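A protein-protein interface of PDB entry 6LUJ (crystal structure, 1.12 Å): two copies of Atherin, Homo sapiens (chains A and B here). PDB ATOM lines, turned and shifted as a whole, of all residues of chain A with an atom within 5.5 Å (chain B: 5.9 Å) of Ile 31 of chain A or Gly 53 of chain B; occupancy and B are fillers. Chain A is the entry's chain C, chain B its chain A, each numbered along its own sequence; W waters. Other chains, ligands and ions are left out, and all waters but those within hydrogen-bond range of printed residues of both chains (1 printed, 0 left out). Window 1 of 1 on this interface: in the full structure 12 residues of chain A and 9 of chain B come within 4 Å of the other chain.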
ATOM      1  N   THR A   6      11.070   2.339  23.318  1.00  0.00           N
ATOM      2  CA  THR A   6      10.554   3.089  24.446  1.00  0.00           C
ATOM      3  C   THR A   6      10.465   4.571  24.090  1.00  0.00           C
ATOM      4  O   THR A   6      10.970   5.027  23.056  1.00  0.00           O
ATOM      5  CB  THR A   6      11.493   2.943  25.637  1.00  0.00           C
ATOM      6  OG1 THR A   6      12.755   3.526  25.298  1.00  0.00           O
ATOM      7  CG2 THR A   6      11.688   1.472  26.005  1.00  0.00           C
ATOM      8  N   VAL A   7       9.827   5.336  24.980  1.00  0.00           N
ATOM      9  CA  VAL A   7       9.818   6.790  24.828  1.00  0.00           C
ATOM     10  C   VAL A   7      11.242   7.322  24.724  1.00  0.00           C
ATOM     11  O   VAL A   7      11.551   8.153  23.861  1.00  0.00           O
ATOM     12  CB  VAL A   7       9.031   7.455  25.973  1.00  0.00           C
ATOM     13  CG1 VAL A   7       9.140   8.968  25.867  1.00  0.00           C
ATOM     14  CG2 VAL A   7       7.570   7.018  25.947  1.00  0.00           C
ATOM     15  N   VAL A  10      12.714   6.862  21.348  1.00  0.00           N
ATOM     16  CA  VAL A  10      12.201   7.841  20.395  1.00  0.00           C
ATOM     17  C   VAL A  10      12.892   9.187  20.585  1.00  0.00           C
ATOM     18  O   VAL A  10      13.285   9.844  19.611  1.00  0.00           O
ATOM     19  CB  VAL A  10      10.670   7.939  20.528  1.00  0.00           C
ATOM     20  CG1 VAL A  10      10.133   9.088  19.695  1.00  0.00           C
ATOM     21  CG2 VAL A  10      10.023   6.621  20.128  1.00  0.00           C
ATOM     22  N   ALA A  25       9.714  17.102  23.267  1.00  0.00           N
ATOM     23  CA  ALA A  25       8.262  17.041  23.142  1.00  0.00           C
ATOM     24  C   ALA A  25       7.774  15.607  22.998  1.00  0.00           C
ATOM     25  O   ALA A  25       6.662  15.283  23.437  1.00  0.00           O
ATOM     26  CB  ALA A  25       7.805  17.876  21.951  1.00  0.00           C
ATOM     27  N   PHE A  26       8.573  14.739  22.373  1.00  0.00           N
ATOM     28  CA  PHE A  26       8.210  13.329  22.314  1.00  0.00           C
ATOM     29  C   PHE A  26       8.201  12.710  23.705  1.00  0.00           C
ATOM     30  O   PHE A  26       7.370  11.840  23.994  1.00  0.00           O
ATOM     31  CB  PHE A  26       9.143  12.580  21.357  1.00  0.00           C
ATOM     32  CG  PHE A  26       8.942  12.941  19.907  1.00  0.00           C
ATOM     33  CD1 PHE A  26       9.581  14.037  19.355  1.00  0.00           C
ATOM     34  CD2 PHE A  26       8.108  12.183  19.102  1.00  0.00           C
ATOM     35  CE1 PHE A  26       9.394  14.369  18.035  1.00  0.00           C
ATOM     36  CE2 PHE A  26       7.914  12.509  17.779  1.00  0.00           C
ATOM     37  CZ  PHE A  26       8.557  13.608  17.240  1.00  0.00           C
ATOM     38  N   GLN A  27       9.094  13.160  24.591  1.00  0.00           N
ATOM     39  CA  GLN A  27       9.024  12.731  25.984  1.00  0.00           C
ATOM     40  C   GLN A  27       7.790  13.302  26.668  1.00  0.00           C
ATOM     41  O   GLN A  27       7.049  12.574  27.341  1.00  0.00           O
ATOM     42  CB  GLN A  27      10.292  13.140  26.736  1.00  0.00           C
ATOM     43  CG  GLN A  27      10.260  12.779  28.217  1.00  0.00           C
ATOM     44  CD  GLN A  27      10.123  11.284  28.453  1.00  0.00           C
ATOM     45  OE1 GLN A  27      11.061  10.523  28.218  1.00  0.00           O
ATOM     46  NE2 GLN A  27       8.954  10.857  28.922  1.00  0.00           N
ATOM     47  N   GLN A  29       4.960  14.176  25.485  1.00  0.00           N
ATOM     48  CA  GLN A  29       3.751  13.520  25.001  1.00  0.00           C
ATOM     49  C   GLN A  29       3.798  12.003  25.125  1.00  0.00           C
ATOM     50  O   GLN A  29       2.852  11.331  24.694  1.00  0.00           O
ATOM     51  CB  GLN A  29       3.467  13.922  23.553  1.00  0.00           C
ATOM     52  CG  GLN A  29       3.210  15.409  23.384  1.00  0.00           C
ATOM     53  CD  GLN A  29       2.089  15.915  24.278  1.00  0.00           C
ATOM     54  OE1 GLN A  29       1.020  15.301  24.380  1.00  0.00           O
ATOM     55  NE2 GLN A  29       2.328  17.040  24.934  1.00  0.00           N
ATOM     56  N   GLU A  30       4.867  11.456  25.698  1.00  0.00           N
ATOM     57  CA  GLU A  30       4.988  10.017  25.939  1.00  0.00           C
ATOM     58  C   GLU A  30       4.815   9.208  24.653  1.00  0.00           C
ATOM     59  O   GLU A  30       4.064   8.232  24.601  1.00  0.00           O
ATOM     60  CB  GLU A  30       4.035   9.548  27.040  1.00  0.00           C
ATOM     61  CG  GLU A  30       4.264  10.244  28.369  1.00  0.00           C
ATOM     62  CD  GLU A  30       5.506   9.756  29.083  1.00  0.00           C
ATOM     63  OE1 GLU A  30       5.953   8.624  28.797  1.00  0.00           O
ATOM     64  OE2 GLU A  30       6.034  10.503  29.936  1.00  0.00           O
ATOM     65  N   ILE A  31       5.521   9.625  23.609  1.00  0.00           N
ATOM     66  CA  ILE A  31       5.485   8.939  22.320  1.00  0.00           C
ATOM     67  C   ILE A  31       6.507   7.812  22.368  1.00  0.00           C
ATOM     68  O   ILE A  31       7.710   8.061  22.273  1.00  0.00           O
ATOM     69  CB  ILE A  31       5.815   9.891  21.164  1.00  0.00           C
ATOM     70  CG1 ILE A  31       4.951  11.157  21.198  1.00  0.00           C
ATOM     71  CG2 ILE A  31       5.748   9.149  19.824  1.00  0.00           C
ATOM     72  CD1 ILE A  31       3.531  10.934  20.804  1.00  0.00           C
ATOM     73  N   ASP A  32       6.035   6.571  22.475  1.00  0.00           N
ATOM     74  CA  ASP A  32       6.904   5.414  22.319  1.00  0.00           C
ATOM     75  C   ASP A  32       6.860   4.938  20.866  1.00  0.00           C
ATOM     76  O   ASP A  32       6.246   5.567  20.005  1.00  0.00           O
ATOM     77  CB  ASP A  32       6.563   4.335  23.346  1.00  0.00           C
ATOM     78  CG  ASP A  32       5.175   3.741  23.150  1.00  0.00           C
ATOM     79  OD1 ASP A  32       4.483   4.069  22.166  1.00  0.00           O
ATOM     80  OD2 ASP A  32       4.766   2.928  24.007  1.00  0.00           O
ATOM     81  N   GLY A  33       7.506   3.802  20.584  1.00  0.00           N
ATOM     82  CA  GLY A  33       7.557   3.312  19.216  1.00  0.00           C
ATOM     83  C   GLY A  33       6.192   2.953  18.664  1.00  0.00           C
ATOM     84  O   GLY A  33       5.915   3.167  17.483  1.00  0.00           O
ATOM     85  N   SER A  35       3.279   4.344  19.443  1.00  0.00           N
ATOM     86  CA  SER A  35       2.582   5.588  19.129  1.00  0.00           C
ATOM     87  C   SER A  35       3.208   6.293  17.936  1.00  0.00           C
ATOM     88  O   SER A  35       2.498   6.897  17.128  1.00  0.00           O
ATOM     89  CB  SER A  35       2.634   6.524  20.338  1.00  0.00           C
ATOM     90  OG  SER A  35       1.999   5.961  21.465  1.00  0.00           O
ATOM     91  N   LEU A  36       4.541   6.247  17.828  1.00  0.00           N
ATOM     92  CA  LEU A  36       5.223   6.921  16.731  1.00  0.00           C
ATOM     93  C   LEU A  36       4.696   6.435  15.392  1.00  0.00           C
ATOM     94  O   LEU A  36       4.464   7.230  14.475  1.00  0.00           O
ATOM     95  CB  LEU A  36       6.727   6.678  16.844  1.00  0.00           C
ATOM     96  CG  LEU A  36       7.612   7.351  15.797  1.00  0.00           C
ATOM     97  CD1 LEU A  36       7.488   8.864  15.886  1.00  0.00           C
ATOM     98  CD2 LEU A  36       9.063   6.916  15.961  1.00  0.00           C
ATOM     99  N   MET A  39       1.353   8.158  14.272  1.00  0.00           N
ATOM    100  CA  MET A  39       1.250   9.603  14.106  1.00  0.00           C
ATOM    101  C   MET A  39       0.958   9.973  12.661  1.00  0.00           C
ATOM    102  O   MET A  39       1.528   9.402  11.724  1.00  0.00           O
ATOM    103  CB  MET A  39       2.545  10.276  14.548  1.00  0.00           C
ATOM    104  CG  MET A  39       2.797  10.152  16.027  1.00  0.00           C
ATOM    105  SD  MET A  39       4.263  11.056  16.532  1.00  0.00           S
ATOM    106  CE  MET A  39       3.611  12.716  16.703  1.00  0.00           C
ATOM    107  N   LEU A  48       2.307  18.217  19.208  1.00  0.00           N
ATOM    108  CA  LEU A  48       3.520  18.182  20.013  1.00  0.00           C
ATOM    109  C   LEU A  48       3.880  19.524  20.628  1.00  0.00           C
ATOM    110  O   LEU A  48       4.779  19.573  21.472  1.00  0.00           O
ATOM    111  CB  LEU A  48       4.704  17.714  19.162  1.00  0.00           C
ATOM    112  CG  LEU A  48       4.660  16.278  18.647  1.00  0.00           C
ATOM    113  CD1 LEU A  48       5.814  16.036  17.682  1.00  0.00           C
ATOM    114  CD2 LEU A  48       4.702  15.281  19.796  1.00  0.00           C
ATOM    115  N   ARG B  51      -2.149  13.320  26.891  1.00  0.00           N
ATOM    116  CA  ARG B  51      -0.906  13.224  26.145  1.00  0.00           C
ATOM    117  C   ARG B  51      -1.102  12.411  24.870  1.00  0.00           C
ATOM    118  O   ARG B  51      -1.862  11.438  24.828  1.00  0.00           O
ATOM    119  CB  ARG B  51       0.191  12.625  27.018  1.00  0.00           C
ATOM    120  CG  ARG B  51       0.733  13.625  28.016  1.00  0.00           C
ATOM    121  CD  ARG B  51       1.603  12.965  29.061  1.00  0.00           C
ATOM    122  NE  ARG B  51       0.796  12.319  30.088  1.00  0.00           N
ATOM    123  CZ  ARG B  51       1.291  11.745  31.179  1.00  0.00           C
ATOM    124  NH1 ARG B  51       2.602  11.729  31.391  1.00  0.00           N
ATOM    125  NH2 ARG B  51       0.474  11.183  32.061  1.00  0.00           N
ATOM    126  N   LEU B  52      -0.380  12.821  23.825  1.00  0.00           N
ATOM    127  CA  LEU B  52      -0.646  12.333  22.478  1.00  0.00           C
ATOM    128  C   LEU B  52      -0.291  10.859  22.305  1.00  0.00           C
ATOM    129  O   LEU B  52      -0.998  10.134  21.598  1.00  0.00           O
ATOM    130  CB  LEU B  52       0.111  13.204  21.479  1.00  0.00           C
ATOM    131  CG  LEU B  52      -0.033  12.881  19.997  1.00  0.00           C
ATOM    132  CD1 LEU B  52      -1.483  12.955  19.560  1.00  0.00           C
ATOM    133  CD2 LEU B  52       0.830  13.839  19.189  1.00  0.00           C
ATOM    134  N   GLY B  53       0.812  10.402  22.889  1.00  0.00           N
ATOM    135  CA  GLY B  53       1.210   9.017  22.751  1.00  0.00           C
ATOM    136  C   GLY B  53       0.137   8.064  23.238  1.00  0.00           C
ATOM    137  O   GLY B  53      -0.349   7.199  22.500  1.00  0.00           O
ATOM    138  N   PRO B  54      -0.249   8.210  24.507  1.00  0.00           N
ATOM    139  CA  PRO B  54      -1.373   7.414  25.018  1.00  0.00           C
ATOM    140  C   PRO B  54      -2.652   7.602  24.223  1.00  0.00           C
ATOM    141  O   PRO B  54      -3.360   6.620  23.969  1.00  0.00           O
ATOM    142  CB  PRO B  54      -1.498   7.890  26.473  1.00  0.00           C
ATOM    143  CG  PRO B  54      -0.103   8.344  26.827  1.00  0.00           C
ATOM    144  CD  PRO B  54       0.428   8.964  25.575  1.00  0.00           C
ATOM    145  N   ALA B  55      -2.962   8.835  23.813  1.00  0.00           N
ATOM    146  CA  ALA B  55      -4.188   9.089  23.057  1.00  0.00           C
ATOM    147  C   ALA B  55      -4.240   8.276  21.771  1.00  0.00           C
ATOM    148  O   ALA B  55      -5.294   7.734  21.411  1.00  0.00           O
ATOM    149  CB  ALA B  55      -4.295  10.581  22.744  1.00  0.00           C
ATOM    150  N   LEU B  56      -3.119   8.203  21.046  1.00  0.00           N
ATOM    151  CA  LEU B  56      -3.084   7.455  19.793  1.00  0.00           C
ATOM    152  C   LEU B  56      -3.396   5.985  20.024  1.00  0.00           C
ATOM    153  O   LEU B  56      -4.161   5.376  19.267  1.00  0.00           O
ATOM    154  CB  LEU B  56      -1.718   7.614  19.129  1.00  0.00           C
ATOM    155  CG  LEU B  56      -1.462   8.991  18.510  1.00  0.00           C
ATOM    156  CD1 LEU B  56       0.032   9.260  18.350  1.00  0.00           C
ATOM    157  CD2 LEU B  56      -2.184   9.121  17.186  1.00  0.00           C
ATOM    158  N   LYS B  57      -2.807   5.404  21.068  1.00  0.00           N
ATOM    159  CA  LYS B  57      -3.066   4.006  21.388  1.00  0.00           C
ATOM    160  C   LYS B  57      -4.491   3.808  21.885  1.00  0.00           C
ATOM    161  O   LYS B  57      -5.157   2.832  21.511  1.00  0.00           O
ATOM    162  CB  LYS B  57      -2.055   3.535  22.432  1.00  0.00           C
ATOM    163  CG  LYS B  57      -0.654   3.412  21.867  1.00  0.00           C
ATOM    164  CD  LYS B  57       0.424   3.710  22.883  1.00  0.00           C
ATOM    165  CE  LYS B  57       0.488   2.674  23.976  1.00  0.00           C
ATOM    166  NZ  LYS B  57       1.771   2.811  24.727  1.00  0.00           N
ATOM    167  N   ILE B  58      -4.969   4.728  22.727  1.00  0.00           N
ATOM    168  CA  ILE B  58      -6.339   4.658  23.228  1.00  0.00           C
ATOM    169  C   ILE B  58      -7.327   4.599  22.071  1.00  0.00           C
ATOM    170  O   ILE B  58      -8.229   3.748  22.042  1.00  0.00           O
ATOM    171  CB  ILE B  58      -6.615   5.838  24.176  1.00  0.00           C
ATOM    172  CG1 ILE B  58      -5.979   5.565  25.538  1.00  0.00           C
ATOM    173  CG2 ILE B  58      -8.110   6.104  24.306  1.00  0.00           C
ATOM    174  CD1 ILE B  58      -5.844   6.788  26.416  1.00  0.00           C
HETATM  175  O   HOH W   1       4.871  13.174  30.098  1.00  0.00           O
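Val 7 of chain A touches none of the printed residues of chain B.
Ala 25 of chain A touches none of the printed residues of chain B.
Ile 31 of chain A touches one residue of chain B.
Of the printed residues of chain B, Ser 35 of chain A touches Gly 53, Leu 56 and Lys 57.
Of the printed residues of chain B, Met 39 of chain A touches Leu 52 and Leu 56.
Of the printed residues of chain A, Gly 53 of chain B touches Gln 29 (2.9 Å), Glu 30 (3.5 Å), Ile 31 (3.5 Å) and Ser 35 (2.8 Å).
Of the printed residues of chain A, Leu 56 of chain B touches Ser 35 (3.6 Å) and Met 39 (3.7 Å).
Of the printed residues of chain A, Lys 57 of chain B touches Asp 32 (3.1 Å) and Ser 35 (3.1 Å).
The nearest residue of chain B that does not touch Ile 31 of chain A is Leu 52 of chain B (4.1 Å).
The nearest printed residue of chain A that does not touch Arg 51 of chain B is Gln 27 of chain A (5.7 Å).
Among the printed residues, pairs that only touch across the chains: Ser 35 of chain A with Lys 57 of chain B (3.1 Å), Gln 29 of chain A with Arg 51 of chain B (3.3 Å), Ile 31 of chain A with Gly 53 of chain B (3.5 Å), Glu 30 of chain A with Gly 53 of chain B (3.5 Å), Gln 29 of chain A with Pro 54 of chain B (3.5 Å), Ser 35 of chain A with Leu 56 of chain B (3.6 Å), Met 39 of chain A with Leu 56 of chain B (3.7 Å), Glu 30 of chain A with Pro 54 of chain B (3.8 Å) and Met 39 of chain A with Leu 52 of chain B (3.9 Å).
The backbone NH (N) of Ser 35 of chain A is in hydrogen-bond range of the side-chain carboxylate (OD1) of Asp 32 of chain A (3.0 Å).
NE2 of Gln 27 of chain A sits at hydrogen-bond distance from OE2 of Glu 30 of chain A (3.1 Å).
N of Ile 31 of chain A lies within hydrogen-bond range of O of Phe 26 of chain A (2.9 Å).
No position is printed for both chains.
Of the 14 pairs that touch across the chains among the printed residues, none has its exchanged pair printed and touching as well.
The guanidinium group of Arg 51 of chain B is in salt-bridge range of the side-chain carboxylate of Glu 30 of chain A, at 3.9 Å.
NZ of Lys 57 of chain B lies within salt-bridge range of OD2 of Asp 32 of chain A.
The backbone NH (N) of Gly 53 of chain B is in hydrogen-bond range of the backbone carbonyl oxygen (O) of Gln 29 of chain A (2.9 Å).
The backbone carbonyl oxygen (O) of Gly 53 of chain B lies within hydrogen-bond range of the side-chain hydroxyl (OG) of Ser 35 of chain A, at 2.8 Å.
N of Leu 52 of chain B is in hydrogen-bond range of OE1 of Gln 29 of chain A.
Of the 15 printed residues of chain A, 6 touch a printed residue of chain B.
Printed residues of chain A that touch a printed residue of chain B: Gln 29, Glu 30, Ile 31, Asp 32, Ser 35 and Met 39.
Hydrophobic or aromatic side chains of chain A within 4 Å of the printed part of chain B: Ile 31 and Met 39.
Of the 8 printed residues of chain B, 6 touch a printed residue of chain A.
Hydrophobic or aromatic side chains of chain B within 4 Å of the printed part of chain A: Leu 52, Pro 54 and Leu 56.
Water W1 bridges the side-chain carboxylate of Glu 30 of chain A (2.9 Å) and the guanidinium group of Arg 51 of chain B (3.0 Å).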
